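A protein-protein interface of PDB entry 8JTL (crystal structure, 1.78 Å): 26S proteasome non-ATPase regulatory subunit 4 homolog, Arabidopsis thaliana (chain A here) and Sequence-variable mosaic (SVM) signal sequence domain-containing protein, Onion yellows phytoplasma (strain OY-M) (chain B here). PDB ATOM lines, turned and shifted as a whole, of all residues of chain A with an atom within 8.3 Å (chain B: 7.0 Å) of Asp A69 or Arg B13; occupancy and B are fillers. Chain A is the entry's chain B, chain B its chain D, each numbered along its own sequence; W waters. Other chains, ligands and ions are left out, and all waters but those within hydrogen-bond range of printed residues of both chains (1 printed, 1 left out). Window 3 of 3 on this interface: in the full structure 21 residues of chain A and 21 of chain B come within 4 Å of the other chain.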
ATOM      1  N   CYS A  38      24.449  12.372 -10.468  1.00  0.00           N
ATOM      2  CA  CYS A  38      23.650  12.139 -11.668  1.00  0.00           C
ATOM      3  C   CYS A  38      22.642  11.047 -11.438  1.00  0.00           C
ATOM      4  O   CYS A  38      21.488  11.150 -11.878  1.00  0.00           O
ATOM      5  CB  CYS A  38      24.532  11.770 -12.864  1.00  0.00           C
ATOM      6  SG  CYS A  38      25.644  13.072 -13.259  1.00  0.00           S
ATOM      7  N   THR A  42      18.692  11.911 -11.454  1.00  0.00           N
ATOM      8  CA  THR A  42      17.859  11.323 -12.491  1.00  0.00           C
ATOM      9  C   THR A  42      16.825  10.386 -11.907  1.00  0.00           C
ATOM     10  O   THR A  42      15.729  10.256 -12.454  1.00  0.00           O
ATOM     11  CB  THR A  42      18.697  10.570 -13.529  1.00  0.00           C
ATOM     12  OG1 THR A  42      19.535   9.615 -12.860  1.00  0.00           O
ATOM     13  CG2 THR A  42      19.532  11.563 -14.333  1.00  0.00           C
ATOM     14  N   GLN A  43      17.140   9.749 -10.790  1.00  0.00           N
ATOM     15  CA  GLN A  43      16.214   8.792 -10.225  1.00  0.00           C
ATOM     16  C   GLN A  43      15.216   9.429  -9.279  1.00  0.00           C
ATOM     17  O   GLN A  43      14.161   8.835  -9.049  1.00  0.00           O
ATOM     18  CB  GLN A  43      16.972   7.691  -9.497  1.00  0.00           C
ATOM     19  CG  GLN A  43      17.968   6.935 -10.420  1.00  0.00           C
ATOM     20  CD  GLN A  43      17.367   6.552 -11.769  1.00  0.00           C
ATOM     21  OE1 GLN A  43      16.450   5.721 -11.824  1.00  0.00           O
ATOM     22  NE2 GLN A  43      17.911   7.110 -12.867  1.00  0.00           N
ATOM     23  N   PRO A  46      11.739  11.135 -12.761  1.00  0.00           N
ATOM     24  CA  PRO A  46      12.005  10.730 -14.148  1.00  0.00           C
ATOM     25  C   PRO A  46      12.054  11.877 -15.121  1.00  0.00           C
ATOM     26  O   PRO A  46      12.574  11.695 -16.225  1.00  0.00           O
ATOM     27  CB  PRO A  46      10.844   9.790 -14.487  1.00  0.00           C
ATOM     28  CG  PRO A  46       9.907   9.860 -13.353  1.00  0.00           C
ATOM     29  CD  PRO A  46      10.480  10.595 -12.223  1.00  0.00           C
ATOM     30  N   ASN A  48      13.576  14.736 -14.243  1.00  0.00           N
ATOM     31  CA  ASN A  48      14.757  15.512 -13.969  1.00  0.00           C
ATOM     32  C   ASN A  48      15.692  15.355 -15.139  1.00  0.00           C
ATOM     33  O   ASN A  48      15.734  14.308 -15.786  1.00  0.00           O
ATOM     34  CB  ASN A  48      15.454  15.048 -12.708  1.00  0.00           C
ATOM     35  CG  ASN A  48      14.785  15.542 -11.475  1.00  0.00           C
ATOM     36  OD1 ASN A  48      13.855  16.348 -11.552  1.00  0.00           O
ATOM     37  ND2 ASN A  48      15.225  15.061 -10.332  1.00  0.00           N
ATOM     38  N   THR A  49      16.457  16.389 -15.405  1.00  0.00           N
ATOM     39  CA  THR A  49      17.497  16.306 -16.408  1.00  0.00           C
ATOM     40  C   THR A  49      18.781  16.764 -15.764  1.00  0.00           C
ATOM     41  O   THR A  49      18.783  17.615 -14.874  1.00  0.00           O
ATOM     42  CB  THR A  49      17.177  17.138 -17.632  1.00  0.00           C
ATOM     43  OG1 THR A  49      16.829  18.472 -17.226  1.00  0.00           O
ATOM     44  CG2 THR A  49      16.030  16.513 -18.397  1.00  0.00           C
ATOM     45  N   VAL A  50      19.863  16.176 -16.208  1.00  0.00           N
ATOM     46  CA  VAL A  50      21.179  16.464 -15.684  1.00  0.00           C
ATOM     47  C   VAL A  50      22.080  16.676 -16.873  1.00  0.00           C
ATOM     48  O   VAL A  50      22.038  15.906 -17.834  1.00  0.00           O
ATOM     49  CB  VAL A  50      21.692  15.325 -14.798  1.00  0.00           C
ATOM     50  CG1 VAL A  50      23.056  15.676 -14.234  1.00  0.00           C
ATOM     51  CG2 VAL A  50      20.719  15.093 -13.687  1.00  0.00           C
ATOM     52  N   GLY A  51      22.826  17.775 -16.861  1.00  0.00           N
ATOM     53  CA  GLY A  51      23.861  18.005 -17.832  1.00  0.00           C
ATOM     54  C   GLY A  51      25.159  18.143 -17.068  1.00  0.00           C
ATOM     55  O   GLY A  51      25.185  18.287 -15.835  1.00  0.00           O
ATOM     56  N   THR A  64      27.345  17.239 -21.794  1.00  0.00           N
ATOM     57  CA  THR A  64      26.005  17.077 -22.299  1.00  0.00           C
ATOM     58  C   THR A  64      25.183  18.205 -21.712  1.00  0.00           C
ATOM     59  O   THR A  64      25.349  18.552 -20.543  1.00  0.00           O
ATOM     60  CB  THR A  64      25.395  15.707 -21.938  1.00  0.00           C
ATOM     61  OG1 THR A  64      24.036  15.672 -22.406  1.00  0.00           O
ATOM     62  CG2 THR A  64      25.406  15.470 -20.417  1.00  0.00           C
ATOM     63  N   THR A  65      24.314  18.780 -22.532  1.00  0.00           N
ATOM     64  CA  THR A  65      23.264  19.595 -21.976  1.00  0.00           C
ATOM     65  C   THR A  65      22.358  18.706 -21.134  1.00  0.00           C
ATOM     66  O   THR A  65      22.367  17.478 -21.290  1.00  0.00           O
ATOM     67  CB  THR A  65      22.457  20.286 -23.076  1.00  0.00           C
ATOM     68  OG1 THR A  65      21.891  19.283 -23.920  1.00  0.00           O
ATOM     69  CG2 THR A  65      23.344  21.201 -23.869  1.00  0.00           C
ATOM     70  N   PRO A  66      21.568  19.303 -20.244  1.00  0.00           N
ATOM     71  CA  PRO A  66      20.771  18.486 -19.331  1.00  0.00           C
ATOM     72  C   PRO A  66      19.917  17.493 -20.089  1.00  0.00           C
ATOM     73  O   PRO A  66      19.294  17.808 -21.112  1.00  0.00           O
ATOM     74  CB  PRO A  66      19.937  19.514 -18.566  1.00  0.00           C
ATOM     75  CG  PRO A  66      20.849  20.710 -18.520  1.00  0.00           C
ATOM     76  CD  PRO A  66      21.561  20.720 -19.850  1.00  0.00           C
ATOM     77  N   THR A  67      19.931  16.268 -19.601  1.00  0.00           N
ATOM     78  CA  THR A  67      19.228  15.200 -20.268  1.00  0.00           C
ATOM     79  C   THR A  67      18.754  14.261 -19.181  1.00  0.00           C
ATOM     80  O   THR A  67      19.307  14.227 -18.090  1.00  0.00           O
ATOM     81  CB  THR A  67      20.124  14.477 -21.291  1.00  0.00           C
ATOM     82  OG1 THR A  67      19.438  13.336 -21.783  1.00  0.00           O
ATOM     83  CG2 THR A  67      21.403  14.008 -20.641  1.00  0.00           C
ATOM     84  N   SER A  68      17.687  13.548 -19.479  1.00  0.00           N
ATOM     85  CA  SER A  68      17.218  12.488 -18.615  1.00  0.00           C
ATOM     86  C   SER A  68      17.941  11.182 -18.883  1.00  0.00           C
ATOM     87  O   SER A  68      17.699  10.195 -18.173  1.00  0.00           O
ATOM     88  CB  SER A  68      15.724  12.300 -18.846  1.00  0.00           C
ATOM     89  OG  SER A  68      15.238  11.237 -18.064  1.00  0.00           O
ATOM     90  N   ASP A  69      18.790  11.158 -19.899  1.00  0.00           N
ATOM     91  CA  ASP A  69      19.399   9.920 -20.381  1.00  0.00           C
ATOM     92  C   ASP A  69      20.608   9.648 -19.503  1.00  0.00           C
ATOM     93  O   ASP A  69      21.679  10.226 -19.691  1.00  0.00           O
ATOM     94  CB  ASP A  69      19.775  10.090 -21.842  1.00  0.00           C
ATOM     95  CG  ASP A  69      20.324   8.839 -22.463  1.00  0.00           C
ATOM     96  OD1 ASP A  69      20.974   8.014 -21.796  1.00  0.00           O
ATOM     97  OD2 ASP A  69      20.098   8.724 -23.684  1.00  0.00           O
ATOM     98  N   LEU A  70      20.430   8.795 -18.508  1.00  0.00           N
ATOM     99  CA  LEU A  70      21.455   8.627 -17.496  1.00  0.00           C
ATOM    100  C   LEU A  70      22.700   8.005 -18.098  1.00  0.00           C
ATOM    101  O   LEU A  70      23.828   8.385 -17.749  1.00  0.00           O
ATOM    102  CB  LEU A  70      20.930   7.770 -16.354  1.00  0.00           C
ATOM    103  CG  LEU A  70      21.935   7.486 -15.219  1.00  0.00           C
ATOM    104  CD1 LEU A  70      22.452   8.760 -14.624  1.00  0.00           C
ATOM    105  CD2 LEU A  70      21.305   6.618 -14.136  1.00  0.00           C
ATOM    106  N   GLY A  71      22.514   7.062 -19.022  1.00  0.00           N
ATOM    107  CA  GLY A  71      23.669   6.469 -19.674  1.00  0.00           C
ATOM    108  C   GLY A  71      24.483   7.502 -20.410  1.00  0.00           C
ATOM    109  O   GLY A  71      25.714   7.537 -20.303  1.00  0.00           O
ATOM    110  N   LYS A  72      23.797   8.403 -21.112  1.00  0.00           N
ATOM    111  CA  LYS A  72      24.477   9.481 -21.807  1.00  0.00           C
ATOM    112  C   LYS A  72      25.229  10.369 -20.831  1.00  0.00           C
ATOM    113  O   LYS A  72      26.392  10.706 -21.061  1.00  0.00           O
ATOM    114  CB  LYS A  72      23.457  10.268 -22.623  1.00  0.00           C
ATOM    115  CG  LYS A  72      23.995  11.480 -23.359  1.00  0.00           C
ATOM    116  CD  LYS A  72      22.849  12.063 -24.181  1.00  0.00           C
ATOM    117  CE  LYS A  72      23.367  13.019 -25.232  1.00  0.00           C
ATOM    118  NZ  LYS A  72      24.471  13.862 -24.643  1.00  0.00           N
ATOM    119  N   ILE A  73      24.591  10.729 -19.711  1.00  0.00           N
ATOM    120  CA  ILE A  73      25.263  11.536 -18.701  1.00  0.00           C
ATOM    121  C   ILE A  73      26.521  10.847 -18.215  1.00  0.00           C
ATOM    122  O   ILE A  73      27.612  11.428 -18.193  1.00  0.00           O
ATOM    123  CB  ILE A  73      24.316  11.789 -17.519  1.00  0.00           C
ATOM    124  CG1 ILE A  73      23.109  12.565 -18.016  1.00  0.00           C
ATOM    125  CG2 ILE A  73      25.083  12.498 -16.443  1.00  0.00           C
ATOM    126  CD1 ILE A  73      21.866  12.329 -17.192  1.00  0.00           C
ATOM    127  N   LEU A  74      26.350   9.633 -17.715  1.00  0.00           N
ATOM    128  CA  LEU A  74      27.445   8.923 -17.095  1.00  0.00           C
ATOM    129  C   LEU A  74      28.546   8.645 -18.101  1.00  0.00           C
ATOM    130  O   LEU A  74      29.727   8.684 -17.749  1.00  0.00           O
ATOM    131  CB  LEU A  74      26.917   7.630 -16.503  1.00  0.00           C
ATOM    132  CG  LEU A  74      25.988   7.863 -15.325  1.00  0.00           C
ATOM    133  CD1 LEU A  74      25.529   6.489 -14.765  1.00  0.00           C
ATOM    134  CD2 LEU A  74      26.734   8.672 -14.281  1.00  0.00           C
ATOM    135  N   ALA A  75      28.182   8.428 -19.352  1.00  0.00           N
ATOM    136  CA  ALA A  75      29.199   8.185 -20.370  1.00  0.00           C
ATOM    137  C   ALA A  75      30.091   9.407 -20.539  1.00  0.00           C
ATOM    138  O   ALA A  75      31.252   9.263 -20.922  1.00  0.00           O
ATOM    139  CB  ALA A  75      28.538   7.803 -21.686  1.00  0.00           C
ATOM    140  N   CYS A  76      29.593  10.576 -20.162  1.00  0.00           N
ATOM    141  CA  CYS A  76      30.395  11.789 -20.219  1.00  0.00           C
ATOM    142  C   CYS A  76      31.478  11.812 -19.184  1.00  0.00           C
ATOM    143  O   CYS A  76      32.439  12.520 -19.335  1.00  0.00           O
ATOM    144  CB  CYS A  76      29.506  13.024 -20.018  1.00  0.00           C
ATOM    145  SG  CYS A  76      28.321  13.292 -21.309  1.00  0.00           S
ATOM    146  N   GLU B   6      33.234   7.612 -26.587  1.00  0.00           N
ATOM    147  CA  GLU B   6      32.079   6.738 -26.667  1.00  0.00           C
ATOM    148  C   GLU B   6      32.542   5.305 -26.790  1.00  0.00           C
ATOM    149  O   GLU B   6      33.490   4.990 -27.502  1.00  0.00           O
ATOM    150  CB  GLU B   6      31.095   7.045 -27.823  1.00  0.00           C
ATOM    151  CG  GLU B   6      31.526   6.654 -29.191  1.00  0.00           C
ATOM    152  CD  GLU B   6      30.398   6.806 -30.232  1.00  0.00           C
ATOM    153  OE1 GLU B   6      29.249   7.118 -29.843  1.00  0.00           O
ATOM    154  OE2 GLU B   6      30.662   6.578 -31.440  1.00  0.00           O
ATOM    155  N   GLU B   7      31.887   4.448 -26.059  1.00  0.00           N
ATOM    156  CA  GLU B   7      32.037   3.031 -26.275  1.00  0.00           C
ATOM    157  C   GLU B   7      30.641   2.514 -26.519  1.00  0.00           C
ATOM    158  O   GLU B   7      29.702   2.903 -25.823  1.00  0.00           O
ATOM    159  CB  GLU B   7      32.674   2.308 -25.091  1.00  0.00           C
ATOM    160  CG  GLU B   7      32.978   0.889 -25.510  1.00  0.00           C
ATOM    161  CD  GLU B   7      33.552   0.033 -24.441  1.00  0.00           C
ATOM    162  OE1 GLU B   7      33.816   0.579 -23.352  1.00  0.00           O
ATOM    163  OE2 GLU B   7      33.715  -1.194 -24.690  1.00  0.00           O
ATOM    164  N   ARG B   8      30.497   1.654 -27.517  1.00  0.00           N
ATOM    165  CA  ARG B   8      29.165   1.174 -27.797  1.00  0.00           C
ATOM    166  C   ARG B   8      29.254  -0.133 -28.559  1.00  0.00           C
ATOM    167  O   ARG B   8      30.265  -0.457 -29.194  1.00  0.00           O
ATOM    168  CB  ARG B   8      28.337   2.228 -28.555  1.00  0.00           C
ATOM    169  CG  ARG B   8      28.645   2.480 -30.032  1.00  0.00           C
ATOM    170  CD  ARG B   8      27.594   3.521 -30.510  1.00  0.00           C
ATOM    171  NE  ARG B   8      27.170   4.392 -29.402  1.00  0.00           N
ATOM    172  CZ  ARG B   8      25.914   4.656 -29.032  1.00  0.00           C
ATOM    173  NH1 ARG B   8      24.874   4.086 -29.623  1.00  0.00           N
ATOM    174  NH2 ARG B   8      25.697   5.460 -27.999  1.00  0.00           N
ATOM    175  N   VAL B   9      28.164  -0.879 -28.473  1.00  0.00           N
ATOM    176  CA  VAL B   9      27.917  -2.012 -29.343  1.00  0.00           C
ATOM    177  C   VAL B   9      26.547  -1.784 -29.950  1.00  0.00           C
ATOM    178  O   VAL B   9      25.541  -1.832 -29.237  1.00  0.00           O
ATOM    179  CB  VAL B   9      27.959  -3.340 -28.598  1.00  0.00           C
ATOM    180  CG1 VAL B   9      27.405  -4.472 -29.522  1.00  0.00           C
ATOM    181  CG2 VAL B   9      29.370  -3.598 -28.117  1.00  0.00           C
ATOM    182  N   GLY B  10      26.510  -1.544 -31.258  1.00  0.00           N
ATOM    183  CA  GLY B  10      25.278  -1.233 -31.944  1.00  0.00           C
ATOM    184  C   GLY B  10      24.590  -0.066 -31.281  1.00  0.00           C
ATOM    185  O   GLY B  10      25.180   0.993 -31.092  1.00  0.00           O
ATOM    186  N   ASP B  11      23.347  -0.279 -30.897  1.00  0.00           N
ATOM    187  CA  ASP B  11      22.543   0.751 -30.261  1.00  0.00           C
ATOM    188  C   ASP B  11      22.869   0.909 -28.793  1.00  0.00           C
ATOM    189  O   ASP B  11      22.381   1.841 -28.156  1.00  0.00           O
ATOM    190  CB  ASP B  11      21.077   0.390 -30.411  1.00  0.00           C
ATOM    191  CG  ASP B  11      20.583   0.591 -31.807  1.00  0.00           C
ATOM    192  OD1 ASP B  11      20.889   1.659 -32.384  1.00  0.00           O
ATOM    193  OD2 ASP B  11      19.939  -0.345 -32.346  1.00  0.00           O
ATOM    194  N   MET B  12      23.652   0.011 -28.228  1.00  0.00           N
ATOM    195  CA  MET B  12      23.869   0.016 -26.798  1.00  0.00           C
ATOM    196  C   MET B  12      25.124   0.762 -26.432  1.00  0.00           C
ATOM    197  O   MET B  12      26.224   0.410 -26.856  1.00  0.00           O
ATOM    198  CB  MET B  12      23.822  -1.388 -26.209  1.00  0.00           C
ATOM    199  CG  MET B  12      24.135  -1.396 -24.730  1.00  0.00           C
ATOM    200  SD  MET B  12      24.324  -3.107 -24.315  1.00  0.00           S
ATOM    201  CE  MET B  12      26.053  -3.528 -24.768  1.00  0.00           C
ATOM    202  N   ARG B  13      24.919   1.795 -25.629  1.00  0.00           N
ATOM    203  CA  ARG B  13      26.016   2.556 -25.097  1.00  0.00           C
ATOM    204  C   ARG B  13      26.689   1.730 -24.031  1.00  0.00           C
ATOM    205  O   ARG B  13      26.030   1.058 -23.228  1.00  0.00           O
ATOM    206  CB  ARG B  13      25.486   3.872 -24.526  1.00  0.00           C
ATOM    207  CG  ARG B  13      26.503   4.713 -23.849  1.00  0.00           C
ATOM    208  CD  ARG B  13      25.803   5.908 -23.223  1.00  0.00           C
ATOM    209  NE  ARG B  13      25.185   6.737 -24.252  1.00  0.00           N
ATOM    210  CZ  ARG B  13      23.881   6.910 -24.435  1.00  0.00           C
ATOM    211  NH1 ARG B  13      22.964   6.297 -23.670  1.00  0.00           N
ATOM    212  NH2 ARG B  13      23.480   7.752 -25.381  1.00  0.00           N
ATOM    213  N   ILE B  14      28.008   1.781 -24.007  1.00  0.00           N
ATOM    214  CA  ILE B  14      28.759   1.142 -22.959  1.00  0.00           C
ATOM    215  C   ILE B  14      29.295   2.228 -22.065  1.00  0.00           C
ATOM    216  O   ILE B  14      29.970   3.153 -22.519  1.00  0.00           O
ATOM    217  CB  ILE B  14      29.876   0.266 -23.532  1.00  0.00           C
ATOM    218  CG1 ILE B  14      29.189  -0.864 -24.314  1.00  0.00           C
ATOM    219  CG2 ILE B  14      30.777  -0.213 -22.415  1.00  0.00           C
ATOM    220  CD1 ILE B  14      30.169  -1.737 -25.073  1.00  0.00           C
ATOM    221  N   VAL B  15      28.928   2.156 -20.798  1.00  0.00           N
ATOM    222  CA  VAL B  15      29.167   3.237 -19.876  1.00  0.00           C
ATOM    223  C   VAL B  15      30.096   2.689 -18.834  1.00  0.00           C
ATOM    224  O   VAL B  15      29.702   1.848 -18.010  1.00  0.00           O
ATOM    225  CB  VAL B  15      27.874   3.750 -19.243  1.00  0.00           C
ATOM    226  CG1 VAL B  15      28.156   4.969 -18.393  1.00  0.00           C
ATOM    227  CG2 VAL B  15      26.859   4.073 -20.336  1.00  0.00           C
ATOM    228  N   ASP B  70      20.854  -2.194 -18.731  1.00  0.00           N
ATOM    229  CA  ASP B  70      19.740  -1.446 -18.163  1.00  0.00           C
ATOM    230  C   ASP B  70      18.393  -1.874 -18.689  1.00  0.00           C
ATOM    231  O   ASP B  70      17.383  -1.287 -18.273  1.00  0.00           O
ATOM    232  CB  ASP B  70      19.922   0.043 -18.394  1.00  0.00           C
ATOM    233  CG  ASP B  70      19.766   0.443 -19.836  1.00  0.00           C
ATOM    234  OD1 ASP B  70      19.729  -0.407 -20.755  1.00  0.00           O
ATOM    235  OD2 ASP B  70      19.746   1.669 -20.046  1.00  0.00           O
ATOM    236  N   ALA B  93      19.222  -3.881 -24.499  1.00  0.00           N
ATOM    237  CA  ALA B  93      19.606  -2.896 -23.502  1.00  0.00           C
ATOM    238  C   ALA B  93      20.171  -1.673 -24.199  1.00  0.00           C
ATOM    239  O   ALA B  93      20.880  -1.786 -25.195  1.00  0.00           O
ATOM    240  CB  ALA B  93      20.647  -3.445 -22.543  1.00  0.00           C
ATOM    241  N   LYS B  94      19.816  -0.508 -23.696  1.00  0.00           N
ATOM    242  CA  LYS B  94      20.369   0.695 -24.284  1.00  0.00           C
ATOM    243  C   LYS B  94      21.688   1.064 -23.648  1.00  0.00           C
ATOM    244  O   LYS B  94      22.461   1.813 -24.235  1.00  0.00           O
ATOM    245  CB  LYS B  94      19.359   1.840 -24.167  1.00  0.00           C
ATOM    246  CG  LYS B  94      17.994   1.383 -24.696  1.00  0.00           C
ATOM    247  CD  LYS B  94      16.864   1.411 -23.638  1.00  0.00           C
ATOM    248  CE  LYS B  94      15.652   0.525 -24.041  1.00  0.00           C
ATOM    249  NZ  LYS B  94      16.116  -0.883 -24.378  1.00  0.00           N
ATOM    250  N   ASN B  95      21.937   0.579 -22.448  1.00  0.00           N
ATOM    251  CA  ASN B  95      23.160   0.938 -21.756  1.00  0.00           C
ATOM    252  C   ASN B  95      23.689  -0.302 -21.106  1.00  0.00           C
ATOM    253  O   ASN B  95      22.930  -1.082 -20.509  1.00  0.00           O
ATOM    254  CB  ASN B  95      22.918   2.002 -20.704  1.00  0.00           C
ATOM    255  CG  ASN B  95      22.561   3.278 -21.323  1.00  0.00           C
ATOM    256  OD1 ASN B  95      23.427   4.032 -21.685  1.00  0.00           O
ATOM    257  ND2 ASN B  95      21.277   3.488 -21.550  1.00  0.00           N
ATOM    258  N   MET B  96      24.961  -0.505 -21.300  1.00  0.00           N
ATOM    259  CA  MET B  96      25.703  -1.510 -20.581  1.00  0.00           C
ATOM    260  C   MET B  96      26.618  -0.753 -19.664  1.00  0.00           C
ATOM    261  O   MET B  96      27.515  -0.047 -20.119  1.00  0.00           O
ATOM    262  CB  MET B  96      26.474  -2.426 -21.507  1.00  0.00           C
ATOM    263  CG  MET B  96      27.193  -3.491 -20.744  1.00  0.00           C
ATOM    264  SD  MET B  96      28.398  -4.162 -21.888  1.00  0.00           S
ATOM    265  CE  MET B  96      29.136  -5.445 -20.941  1.00  0.00           C
ATOM    266  N   TYR B  97      26.330  -0.827 -18.381  1.00  0.00           N
ATOM    267  CA  TYR B  97      27.151  -0.175 -17.387  1.00  0.00           C
ATOM    268  C   TYR B  97      28.199  -1.149 -16.930  1.00  0.00           C
ATOM    269  O   TYR B  97      27.881  -2.233 -16.436  1.00  0.00           O
ATOM    270  CB  TYR B  97      26.313   0.272 -16.201  1.00  0.00           C
ATOM    271  CG  TYR B  97      25.353   1.316 -16.625  1.00  0.00           C
ATOM    272  CD1 TYR B  97      25.716   2.654 -16.631  1.00  0.00           C
ATOM    273  CD2 TYR B  97      24.090   0.972 -17.069  1.00  0.00           C
ATOM    274  CE1 TYR B  97      24.805   3.647 -17.011  1.00  0.00           C
ATOM    275  CE2 TYR B  97      23.184   1.935 -17.415  1.00  0.00           C
ATOM    276  CZ  TYR B  97      23.534   3.263 -17.397  1.00  0.00           C
ATOM    277  OH  TYR B  97      22.580   4.169 -17.789  1.00  0.00           O
HETATM  278  O   HOH W   1      19.608   5.711 -22.237  1.00  0.00           O
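OD1 of Asp A69 lies within salt-bridge range of NH1 of Arg B13, at 3.2 Å. N of Gly A71 is in hydrogen-bond range of OH of Tyr B97, at 3.1 Å. N of Lys A72 sits close to NH1 of Arg B13 (3.4 Å).
OG1 of Thr A64 lies within hydrogen-bond range of NZ of Lys A72 (2.9 Å). The backbone NH (N) of Asp A69 sits at hydrogen-bond distance from the side-chain hydroxyl (OG1) of Thr A67 (3.0 Å). N of Gly A71 sits close to OD1 of Asp A69, at 3.3 Å. The backbone NH (N) of Arg B13 sits at hydrogen-bond distance from the backbone carbonyl oxygen (O) of Lys B94 (2.8 Å). OD1 of Asn B95 is in hydrogen-bond range of NH1 of Arg B13, at 3.0 Å. ND2 of Asn B95 sits at hydrogen-bond distance from OD2 of Asp B70, 2.8 Å away.
Leu A70 touches Tyr B97 (C to OH, 3.9 Å). Gly A71 touches Arg B13. Val B15 touches Gly A71. CA of Gly A71 touches OD1 of Asn B95, at 3.2 Å. Val B15 touches Leu A74. CE1 of Tyr B97 touches CD1 of Leu A74, 3.7 Å away. Arg B13 touches Ala A75 (CD to CB, 3.7 Å). Ala A75 touches Val B15 (N to CG1, 3.6 Å).
Gly A51 touches none of the printed residues of chain B. Asp A69 touches just one residue of chain B: Arg B13. Of the printed residues of chain B, Gly A71 touches Arg B13 (3.3 Å), Val B15 (3.6 Å), Asn B95 (3.2 Å) and Tyr B97 (3.1 Å). Printed residues of chain B within 4 Å of Lys A72: Arg B13. Of the printed residues of chain B, Leu A74 touches Val B15 and Tyr B97. Of the printed residues of chain B, Ala A75 touches Arg B13 and Val B15. Cys A76 touches none of the printed residues of chain B. Of chain A, only Asp A69 (3.2 Å), Gly A71 (3.3 Å), Lys A72 (3.4 Å) and Ala A75 (3.7 Å) come within 4 Å of Arg B13. The nearest residue of chain A that does not touch Arg B13 is Leu A70 (5.8 Å).
Hydrophobic or aromatic side chains of chain A within 4 Å of the printed part of chain B: Leu A74 and Ala A75. Among the printed residues, Asp or Glu carboxylates within 4 Å of a Lys or Arg side-chain nitrogen of the other chain: Asp A69 with Arg B13.
Water W1 bridges the side-chain carboxylate of Asp A69 (2.7 Å) and the side-chain amide nitrogen of Asn B95 (2.9 Å).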
